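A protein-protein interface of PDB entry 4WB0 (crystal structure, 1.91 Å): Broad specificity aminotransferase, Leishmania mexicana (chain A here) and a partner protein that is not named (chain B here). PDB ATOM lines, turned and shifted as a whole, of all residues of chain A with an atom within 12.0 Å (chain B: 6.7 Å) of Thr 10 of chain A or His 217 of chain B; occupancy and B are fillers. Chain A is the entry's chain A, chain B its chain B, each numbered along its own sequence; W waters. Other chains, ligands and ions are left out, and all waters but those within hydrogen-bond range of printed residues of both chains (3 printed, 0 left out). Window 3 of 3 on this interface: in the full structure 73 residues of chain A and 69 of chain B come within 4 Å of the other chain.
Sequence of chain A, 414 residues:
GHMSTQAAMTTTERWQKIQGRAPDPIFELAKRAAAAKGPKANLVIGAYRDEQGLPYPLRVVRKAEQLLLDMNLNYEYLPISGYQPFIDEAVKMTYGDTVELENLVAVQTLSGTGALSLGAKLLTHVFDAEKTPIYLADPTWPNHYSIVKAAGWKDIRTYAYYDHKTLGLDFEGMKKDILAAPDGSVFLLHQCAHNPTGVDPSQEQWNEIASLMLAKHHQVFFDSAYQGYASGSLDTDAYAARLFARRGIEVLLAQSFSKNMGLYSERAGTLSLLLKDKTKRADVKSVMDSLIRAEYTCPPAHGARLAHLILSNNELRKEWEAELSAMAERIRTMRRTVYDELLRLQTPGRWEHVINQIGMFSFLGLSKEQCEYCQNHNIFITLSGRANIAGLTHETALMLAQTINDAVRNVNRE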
ATOM      1  N   ALA A   8     -25.439  15.225 -15.240  1.00  0.00           N
ATOM      2  CA  ALA A   8     -24.287  15.955 -15.751  1.00  0.00           C
ATOM      3  C   ALA A   8     -24.676  17.275 -16.430  1.00  0.00           C
ATOM      4  O   ALA A   8     -24.270  17.524 -17.566  1.00  0.00           O
ATOM      5  CB  ALA A   8     -23.511  15.085 -16.724  1.00  0.00           C
ATOM      6  N   MET A   9     -25.468  18.102 -15.745  1.00  0.00           N
ATOM      7  CA  MET A   9     -25.723  19.495 -16.171  1.00  0.00           C
ATOM      8  C   MET A   9     -25.939  20.336 -14.901  1.00  0.00           C
ATOM      9  O   MET A   9     -25.109  21.202 -14.593  1.00  0.00           O
ATOM     10  CB  MET A   9     -26.905  19.609 -17.110  1.00  0.00           C
ATOM     11  CG  MET A   9     -27.047  20.986 -17.702  1.00  0.00           C
ATOM     12  SD  MET A   9     -28.749  21.361 -18.027  1.00  0.00           S
ATOM     13  CE  MET A   9     -28.934  20.652 -19.681  1.00  0.00           C
ATOM     14  N   THR A  10     -27.006  20.056 -14.147  1.00  0.00           N
ATOM     15  CA  THR A  10     -27.125  20.590 -12.784  1.00  0.00           C
ATOM     16  C   THR A  10     -26.254  19.825 -11.786  1.00  0.00           C
ATOM     17  O   THR A  10     -25.945  18.653 -12.001  1.00  0.00           O
ATOM     18  CB  THR A  10     -28.538  20.514 -12.254  1.00  0.00           C
ATOM     19  OG1 THR A  10     -28.854  19.139 -12.025  1.00  0.00           O
ATOM     20  CG2 THR A  10     -29.547  21.177 -13.235  1.00  0.00           C
ATOM     21  N   THR A  11     -25.879  20.458 -10.674  1.00  0.00           N
ATOM     22  CA  THR A  11     -25.047  19.732  -9.714  1.00  0.00           C
ATOM     23  C   THR A  11     -25.771  18.499  -9.169  1.00  0.00           C
ATOM     24  O   THR A  11     -25.147  17.471  -8.935  1.00  0.00           O
ATOM     25  CB  THR A  11     -24.560  20.623  -8.529  1.00  0.00           C
ATOM     26  OG1 THR A  11     -25.628  21.355  -7.915  1.00  0.00           O
ATOM     27  CG2 THR A  11     -23.510  21.599  -9.009  1.00  0.00           C
ATOM     28  N   THR A  12     -27.087  18.571  -9.002  1.00  0.00           N
ATOM     29  CA  THR A  12     -27.850  17.403  -8.548  1.00  0.00           C
ATOM     30  C   THR A  12     -27.639  16.194  -9.461  1.00  0.00           C
ATOM     31  O   THR A  12     -27.436  15.085  -8.986  1.00  0.00           O
ATOM     32  CB  THR A  12     -29.351  17.716  -8.480  1.00  0.00           C
ATOM     33  OG1 THR A  12     -29.551  18.859  -7.632  1.00  0.00           O
ATOM     34  CG2 THR A  12     -30.141  16.511  -7.956  1.00  0.00           C
ATOM     35  N   GLU A  13     -27.709  16.434 -10.771  1.00  0.00           N
ATOM     36  CA  GLU A  13     -27.500  15.402 -11.788  1.00  0.00           C
ATOM     37  C   GLU A  13     -26.069  14.815 -11.721  1.00  0.00           C
ATOM     38  O   GLU A  13     -25.875  13.600 -11.886  1.00  0.00           O
ATOM     39  CB  GLU A  13     -27.777  15.991 -13.177  1.00  0.00           C
ATOM     40  CG  GLU A  13     -29.252  16.350 -13.408  1.00  0.00           C
ATOM     41  CD  GLU A  13     -29.484  17.240 -14.644  1.00  0.00           C
ATOM     42  OE1 GLU A  13     -28.903  18.340 -14.728  1.00  0.00           O
ATOM     43  OE2 GLU A  13     -30.250  16.841 -15.533  1.00  0.00           O
ATOM     44  N   ARG A  14     -25.085  15.688 -11.469  1.00  0.00           N
ATOM     45  CA  ARG A  14     -23.676  15.295 -11.341  1.00  0.00           C
ATOM     46  C   ARG A  14     -23.469  14.375 -10.152  1.00  0.00           C
ATOM     47  O   ARG A  14     -22.770  13.359 -10.255  1.00  0.00           O
ATOM     48  CB  ARG A  14     -22.763  16.512 -11.153  1.00  0.00           C
ATOM     49  CG  ARG A  14     -22.879  17.588 -12.203  1.00  0.00           C
ATOM     50  CD  ARG A  14     -21.747  17.531 -13.193  1.00  0.00           C
ATOM     51  NE  ARG A  14     -21.656  18.769 -13.969  1.00  0.00           N
ATOM     52  CZ  ARG A  14     -21.162  18.847 -15.199  1.00  0.00           C
ATOM     53  NH1 ARG A  14     -20.729  17.758 -15.825  1.00  0.00           N
ATOM     54  NH2 ARG A  14     -21.112  20.020 -15.813  1.00  0.00           N
ATOM     55  N   TRP A  15     -24.036  14.754  -9.006  1.00  0.00           N
ATOM     56  CA  TRP A  15     -23.893  13.933  -7.803  1.00  0.00           C
ATOM     57  C   TRP A  15     -24.619  12.615  -7.967  1.00  0.00           C
ATOM     58  O   TRP A  15     -24.136  11.578  -7.514  1.00  0.00           O
ATOM     59  CB  TRP A  15     -24.401  14.662  -6.567  1.00  0.00           C
ATOM     60  CG  TRP A  15     -23.427  15.692  -6.088  1.00  0.00           C
ATOM     61  CD1 TRP A  15     -23.486  17.027  -6.324  1.00  0.00           C
ATOM     62  CD2 TRP A  15     -22.223  15.468  -5.318  1.00  0.00           C
ATOM     63  NE1 TRP A  15     -22.411  17.667  -5.736  1.00  0.00           N
ATOM     64  CE2 TRP A  15     -21.622  16.730  -5.118  1.00  0.00           C
ATOM     65  CE3 TRP A  15     -21.604  14.327  -4.772  1.00  0.00           C
ATOM     66  CZ2 TRP A  15     -20.437  16.892  -4.405  1.00  0.00           C
ATOM     67  CZ3 TRP A  15     -20.410  14.490  -4.053  1.00  0.00           C
ATOM     68  CH2 TRP A  15     -19.843  15.765  -3.876  1.00  0.00           C
ATOM     69  N   GLN A  16     -25.748  12.639  -8.667  1.00  0.00           N
ATOM     70  CA  GLN A  16     -26.513  11.414  -8.872  1.00  0.00           C
ATOM     71  C   GLN A  16     -25.673  10.286  -9.496  1.00  0.00           C
ATOM     72  O   GLN A  16     -25.954   9.120  -9.299  1.00  0.00           O
ATOM     73  CB  GLN A  16     -27.726  11.689  -9.747  1.00  0.00           C
ATOM     74  CG  GLN A  16     -28.721  10.523  -9.787  1.00  0.00           C
ATOM     75  CD  GLN A  16     -29.452  10.295  -8.460  1.00  0.00           C
ATOM     76  OE1 GLN A  16     -29.860  11.254  -7.778  1.00  0.00           O
ATOM     77  NE2 GLN A  16     -29.636   9.014  -8.094  1.00  0.00           N
ATOM     78  N   LYS A  17     -24.651  10.641 -10.258  1.00  0.00           N
ATOM     79  CA  LYS A  17     -23.815   9.659 -10.931  1.00  0.00           C
ATOM     80  C   LYS A  17     -22.590   9.163 -10.132  1.00  0.00           C
ATOM     81  O   LYS A  17     -21.762   8.415 -10.662  1.00  0.00           O
ATOM     82  CB  LYS A  17     -23.358  10.266 -12.239  1.00  0.00           C
ATOM     83  CG  LYS A  17     -24.516  10.528 -13.248  1.00  0.00           C
ATOM     84  CD  LYS A  17     -23.981  11.169 -14.496  1.00  0.00           C
ATOM     85  CE  LYS A  17     -24.958  11.045 -15.654  1.00  0.00           C
ATOM     86  NZ  LYS A  17     -24.287  11.250 -16.979  1.00  0.00           N
ATOM     87  N   ILE A  18     -22.442   9.592  -8.878  1.00  0.00           N
ATOM     88  CA  ILE A  18     -21.286   9.157  -8.098  1.00  0.00           C
ATOM     89  C   ILE A  18     -21.391   7.669  -7.826  1.00  0.00           C
ATOM     90  O   ILE A  18     -22.460   7.145  -7.508  1.00  0.00           O
ATOM     91  CB  ILE A  18     -21.122   9.942  -6.767  1.00  0.00           C
ATOM     92  CG1 ILE A  18     -19.697   9.778  -6.242  1.00  0.00           C
ATOM     93  CG2 ILE A  18     -22.170   9.525  -5.717  1.00  0.00           C
ATOM     94  CD1 ILE A  18     -19.370  10.678  -5.033  1.00  0.00           C
ATOM     95  N   PHE B 127     -16.730  15.336 -10.710  1.00  0.00           N
ATOM     96  CA  PHE B 127     -16.251  16.132 -11.844  1.00  0.00           C
ATOM     97  C   PHE B 127     -14.971  15.557 -12.468  1.00  0.00           C
ATOM     98  O   PHE B 127     -14.224  14.828 -11.808  1.00  0.00           O
ATOM     99  CB  PHE B 127     -16.005  17.584 -11.380  1.00  0.00           C
ATOM    100  CG  PHE B 127     -17.249  18.286 -10.893  1.00  0.00           C
ATOM    101  CD1 PHE B 127     -17.671  18.158  -9.572  1.00  0.00           C
ATOM    102  CD2 PHE B 127     -17.995  19.076 -11.756  1.00  0.00           C
ATOM    103  CE1 PHE B 127     -18.810  18.795  -9.134  1.00  0.00           C
ATOM    104  CE2 PHE B 127     -19.125  19.708 -11.335  1.00  0.00           C
ATOM    105  CZ  PHE B 127     -19.555  19.567 -10.043  1.00  0.00           C
ATOM    106  N   ASP B 183     -19.893  26.454 -17.670  1.00  0.00           N
ATOM    107  CA  ASP B 183     -20.882  25.878 -16.767  1.00  0.00           C
ATOM    108  C   ASP B 183     -20.327  24.666 -16.069  1.00  0.00           C
ATOM    109  O   ASP B 183     -19.539  23.908 -16.640  1.00  0.00           O
ATOM    110  CB  ASP B 183     -22.149  25.448 -17.497  1.00  0.00           C
ATOM    111  CG  ASP B 183     -22.846  26.593 -18.209  1.00  0.00           C
ATOM    112  OD1 ASP B 183     -22.453  27.765 -18.037  1.00  0.00           O
ATOM    113  OD2 ASP B 183     -23.805  26.291 -18.943  1.00  0.00           O
ATOM    114  N   GLY B 184     -20.765  24.465 -14.836  1.00  0.00           N
ATOM    115  CA  GLY B 184     -20.391  23.280 -14.116  1.00  0.00           C
ATOM    116  C   GLY B 184     -18.949  23.265 -13.610  1.00  0.00           C
ATOM    117  O   GLY B 184     -18.371  22.192 -13.502  1.00  0.00           O
ATOM    118  N   SER B 185     -18.379  24.439 -13.314  1.00  0.00           N
ATOM    119  CA  SER B 185     -17.031  24.538 -12.759  1.00  0.00           C
ATOM    120  C   SER B 185     -17.105  24.471 -11.215  1.00  0.00           C
ATOM    121  O   SER B 185     -18.188  24.553 -10.656  1.00  0.00           O
ATOM    122  CB  SER B 185     -16.371  25.839 -13.227  1.00  0.00           C
ATOM    123  OG  SER B 185     -16.076  25.815 -14.624  1.00  0.00           O
ATOM    124  N   LEU B 212     -26.046  33.524  -9.412  1.00  0.00           N
ATOM    125  CA  LEU B 212     -25.121  33.270 -10.497  1.00  0.00           C
ATOM    126  C   LEU B 212     -24.676  31.809 -10.475  1.00  0.00           C
ATOM    127  O   LEU B 212     -24.579  31.150 -11.515  1.00  0.00           O
ATOM    128  CB  LEU B 212     -23.912  34.205 -10.396  1.00  0.00           C
ATOM    129  CG  LEU B 212     -24.113  35.684 -10.766  1.00  0.00           C
ATOM    130  CD1 LEU B 212     -22.755  36.382 -10.653  1.00  0.00           C
ATOM    131  CD2 LEU B 212     -24.715  35.884 -12.136  1.00  0.00           C
ATOM    132  N   MET B 213     -24.394  31.304  -9.279  1.00  0.00           N
ATOM    133  CA  MET B 213     -23.941  29.912  -9.164  1.00  0.00           C
ATOM    134  C   MET B 213     -25.009  28.931  -9.652  1.00  0.00           C
ATOM    135  O   MET B 213     -24.681  27.924 -10.278  1.00  0.00           O
ATOM    136  CB  MET B 213     -23.554  29.595  -7.727  1.00  0.00           C
ATOM    137  CG  MET B 213     -22.329  30.351  -7.279  1.00  0.00           C
ATOM    138  SD  MET B 213     -20.772  29.833  -8.062  1.00  0.00           S
ATOM    139  CE  MET B 213     -19.655  31.090  -7.463  1.00  0.00           C
ATOM    140  N   LEU B 214     -26.276  29.219  -9.374  1.00  0.00           N
ATOM    141  CA  LEU B 214     -27.360  28.353  -9.811  1.00  0.00           C
ATOM    142  C   LEU B 214     -27.502  28.381 -11.340  1.00  0.00           C
ATOM    143  O   LEU B 214     -27.584  27.338 -11.995  1.00  0.00           O
ATOM    144  CB  LEU B 214     -28.697  28.787  -9.191  1.00  0.00           C
ATOM    145  CG  LEU B 214     -28.886  28.491  -7.714  1.00  0.00           C
ATOM    146  CD1 LEU B 214     -30.075  29.316  -7.159  1.00  0.00           C
ATOM    147  CD2 LEU B 214     -29.102  26.989  -7.527  1.00  0.00           C
ATOM    148  N   ALA B 215     -27.559  29.597 -11.881  1.00  0.00           N
ATOM    149  CA  ALA B 215     -27.695  29.798 -13.314  1.00  0.00           C
ATOM    150  C   ALA B 215     -26.563  29.119 -14.097  1.00  0.00           C
ATOM    151  O   ALA B 215     -26.769  28.663 -15.209  1.00  0.00           O
ATOM    152  CB  ALA B 215     -27.721  31.269 -13.618  1.00  0.00           C
ATOM    153  N   LYS B 216     -25.360  29.071 -13.520  1.00  0.00           N
ATOM    154  CA  LYS B 216     -24.216  28.480 -14.215  1.00  0.00           C
ATOM    155  C   LYS B 216     -23.973  27.003 -13.853  1.00  0.00           C
ATOM    156  O   LYS B 216     -23.086  26.354 -14.445  1.00  0.00           O
ATOM    157  CB  LYS B 216     -22.951  29.300 -13.922  1.00  0.00           C
ATOM    158  CG  LYS B 216     -22.951  30.675 -14.575  1.00  0.00           C
ATOM    159  CD  LYS B 216     -22.729  30.557 -16.101  1.00  0.00           C
ATOM    160  CE  LYS B 216     -21.290  30.099 -16.468  1.00  0.00           C
ATOM    161  NZ  LYS B 216     -21.097  30.159 -17.992  1.00  0.00           N
ATOM    162  N   HIS B 217     -24.762  26.480 -12.909  1.00  0.00           N
ATOM    163  CA  HIS B 217     -24.638  25.085 -12.432  1.00  0.00           C
ATOM    164  C   HIS B 217     -23.248  24.783 -11.856  1.00  0.00           C
ATOM    165  O   HIS B 217     -22.757  23.648 -11.925  1.00  0.00           O
ATOM    166  CB  HIS B 217     -24.928  24.090 -13.548  1.00  0.00           C
ATOM    167  CG  HIS B 217     -26.181  24.378 -14.309  1.00  0.00           C
ATOM    168  ND1 HIS B 217     -27.420  23.954 -13.884  1.00  0.00           N
ATOM    169  CD2 HIS B 217     -26.385  25.044 -15.471  1.00  0.00           C
ATOM    170  CE1 HIS B 217     -28.334  24.338 -14.758  1.00  0.00           C
ATOM    171  NE2 HIS B 217     -27.732  25.003 -15.729  1.00  0.00           N
ATOM    172  N   HIS B 218     -22.621  25.808 -11.297  1.00  0.00           N
ATOM    173  CA  HIS B 218     -21.356  25.633 -10.629  1.00  0.00           C
ATOM    174  C   HIS B 218     -21.530  24.861  -9.320  1.00  0.00           C
ATOM    175  O   HIS B 218     -22.548  24.979  -8.626  1.00  0.00           O
ATOM    176  CB  HIS B 218     -20.701  26.983 -10.328  1.00  0.00           C
ATOM    177  CG  HIS B 218     -20.268  27.738 -11.545  1.00  0.00           C
ATOM    178  ND1 HIS B 218     -19.649  27.136 -12.622  1.00  0.00           N
ATOM    179  CD2 HIS B 218     -20.367  29.050 -11.856  1.00  0.00           C
ATOM    180  CE1 HIS B 218     -19.398  28.045 -13.546  1.00  0.00           C
ATOM    181  NE2 HIS B 218     -19.811  29.219 -13.100  1.00  0.00           N
ATOM    182  N   GLN B 219     -20.507  24.090  -8.978  1.00  0.00           N
ATOM    183  CA  GLN B 219     -20.427  23.496  -7.639  1.00  0.00           C
ATOM    184  C   GLN B 219     -19.760  24.463  -6.674  1.00  0.00           C
ATOM    185  O   GLN B 219     -18.651  24.984  -6.935  1.00  0.00           O
ATOM    186  CB  GLN B 219     -19.652  22.189  -7.676  1.00  0.00           C
ATOM    187  CG  GLN B 219     -19.298  21.603  -6.275  1.00  0.00           C
ATOM    188  CD  GLN B 219     -20.500  20.964  -5.644  1.00  0.00           C
ATOM    189  OE1 GLN B 219     -21.182  20.149  -6.274  1.00  0.00           O
ATOM    190  NE2 GLN B 219     -20.804  21.359  -4.417  1.00  0.00           N
ATOM    191  N   GLU B 250     -26.326  22.827  -3.665  1.00  0.00           N
ATOM    192  CA  GLU B 250     -25.732  21.664  -2.993  1.00  0.00           C
ATOM    193  C   GLU B 250     -24.348  22.000  -2.439  1.00  0.00           C
ATOM    194  O   GLU B 250     -23.319  21.756  -3.083  1.00  0.00           O
ATOM    195  CB  GLU B 250     -25.664  20.480  -3.952  1.00  0.00           C
ATOM    196  CG  GLU B 250     -27.032  19.904  -4.215  1.00  0.00           C
ATOM    197  CD  GLU B 250     -27.090  19.051  -5.458  1.00  0.00           C
ATOM    198  OE1 GLU B 250     -26.365  19.353  -6.444  1.00  0.00           O
ATOM    199  OE2 GLU B 250     -27.879  18.077  -5.440  1.00  0.00           O
HETATM  200  O   HOH W   1     -25.574  23.539  -6.584  1.00  0.00           O
HETATM  201  O   HOH W   2     -17.955  20.078 -15.221  1.00  0.00           O
HETATM  202  O   HOH W   3     -23.083  20.953 -12.831  1.00  0.00           O
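The side-chain carboxylate of Glu 250 of chain B lies within hydrogen-bond range of the side-chain hydroxyl of Thr 11 of chain A (2.6 Å). The backbone NH (N) of Thr 12 of chain A sits at hydrogen-bond distance from the side-chain carboxylate (OE1) of Glu 250 of chain B (2.8 Å). The indole nitrogen (NE1) of Trp 15 of chain A lies within hydrogen-bond range of the side-chain amide oxygen (OE1) of Gln 219 of chain B (2.8 Å).
The backbone NH (N) of Thr 10 of chain A is in hydrogen-bond range of the side-chain carboxylate (OE1) of Glu 13 of chain A (2.6 Å). A ring nitrogen (ND1) of His 218 of chain B lies within hydrogen-bond range of the backbone NH (N) of Ser 185 of chain B (3.1 Å). The backbone carbonyl oxygen (O) of Met 213 of chain B lies within hydrogen-bond range of the backbone NH (N) of His 218 of chain B (3.1 Å). O of Ser 185 of chain B lies within hydrogen-bond range of N of Gln 219 of chain B (2.9 Å). The backbone carbonyl oxygen of Glu 250 of chain B is in hydrogen-bond range of the side-chain amide nitrogen of Gln 219 of chain B, 2.9 Å away. The backbone NH (N) of Gly 184 of chain B sits at hydrogen-bond distance from the backbone carbonyl oxygen (O) of Lys 216 of chain B, 3.0 Å away.
Among the printed residues, pairs that only touch across the chains: Met 9 of chain A with His 217 of chain B (3.1 Å), Thr 10 of chain A with His 217 of chain B (3.6 Å), Thr 11 of chain A with His 217 of chain B (3.6 Å), Thr 11 of chain A with His 218 of chain B (3.5 Å), Thr 11 of chain A with Gln 219 of chain B (3.9 Å), Arg 14 of chain A with Phe 127 of chain B (3.8 Å), Arg 14 of chain A with Gly 184 of chain B (3.7 Å) and Trp 15 of chain A with Glu 250 of chain B (3.7 Å).
Thr 10 of chain A touches just one residue of chain B: His 217. Of the printed residues of chain B, Thr 11 of chain A touches His 217, His 218, Gln 219 and Glu 250. Printed residues of chain B within 4 Å of Trp 15 of chain A: Gln 219 and Glu 250. No residue of chain A comes within 4 Å of Asp 183 of chain B. Gly 184 of chain B touches just one residue of chain A: Arg 14. No residue of chain A comes within 4 Å of Ser 185 of chain B. Ala 215 of chain B touches none of the printed residues of chain A. Of the printed residues of chain A, His 217 of chain B touches Met 9, Thr 10 and Thr 11. His 218 of chain B touches one residue of chain A. Of the printed residues of chain A, Glu 250 of chain B touches Thr 11, Thr 12 and Trp 15. The nearest residue of chain A that does not touch His 217 of chain B is Arg 14 of chain A (5.4 Å). The nearest printed residue of chain B that does not touch Trp 15 of chain A is Phe 127 of chain B (5.1 Å).
Hydrophobic or aromatic side chains of chain A within 4 Å of the printed part of chain B: Trp 15. Of the 13 printed residues of chain B, 6 touch a printed residue of chain A. Hydrophobic or aromatic side chains of chain B within 4 Å of the printed part of chain A: Phe 127 and His 217.
Water W1 lies within hydrogen-bond range of the side-chain hydroxyl of Thr 11 of chain A (2.6 Å) and the backbone NH of Glu 250 of chain B (3.1 Å). Water W3 lies within hydrogen-bond range of O of Met 9 of chain A (2.7 Å), NE of Arg 14 of chain A (2.8 Å) and O of His 217 of chain B (2.9 Å). Water W2 lies within hydrogen-bond range of the backbone carbonyl oxygen of Gly 184 of chain B (2.8 Å) and the guanidinium group of Arg 14 of chain A (3.2 Å).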
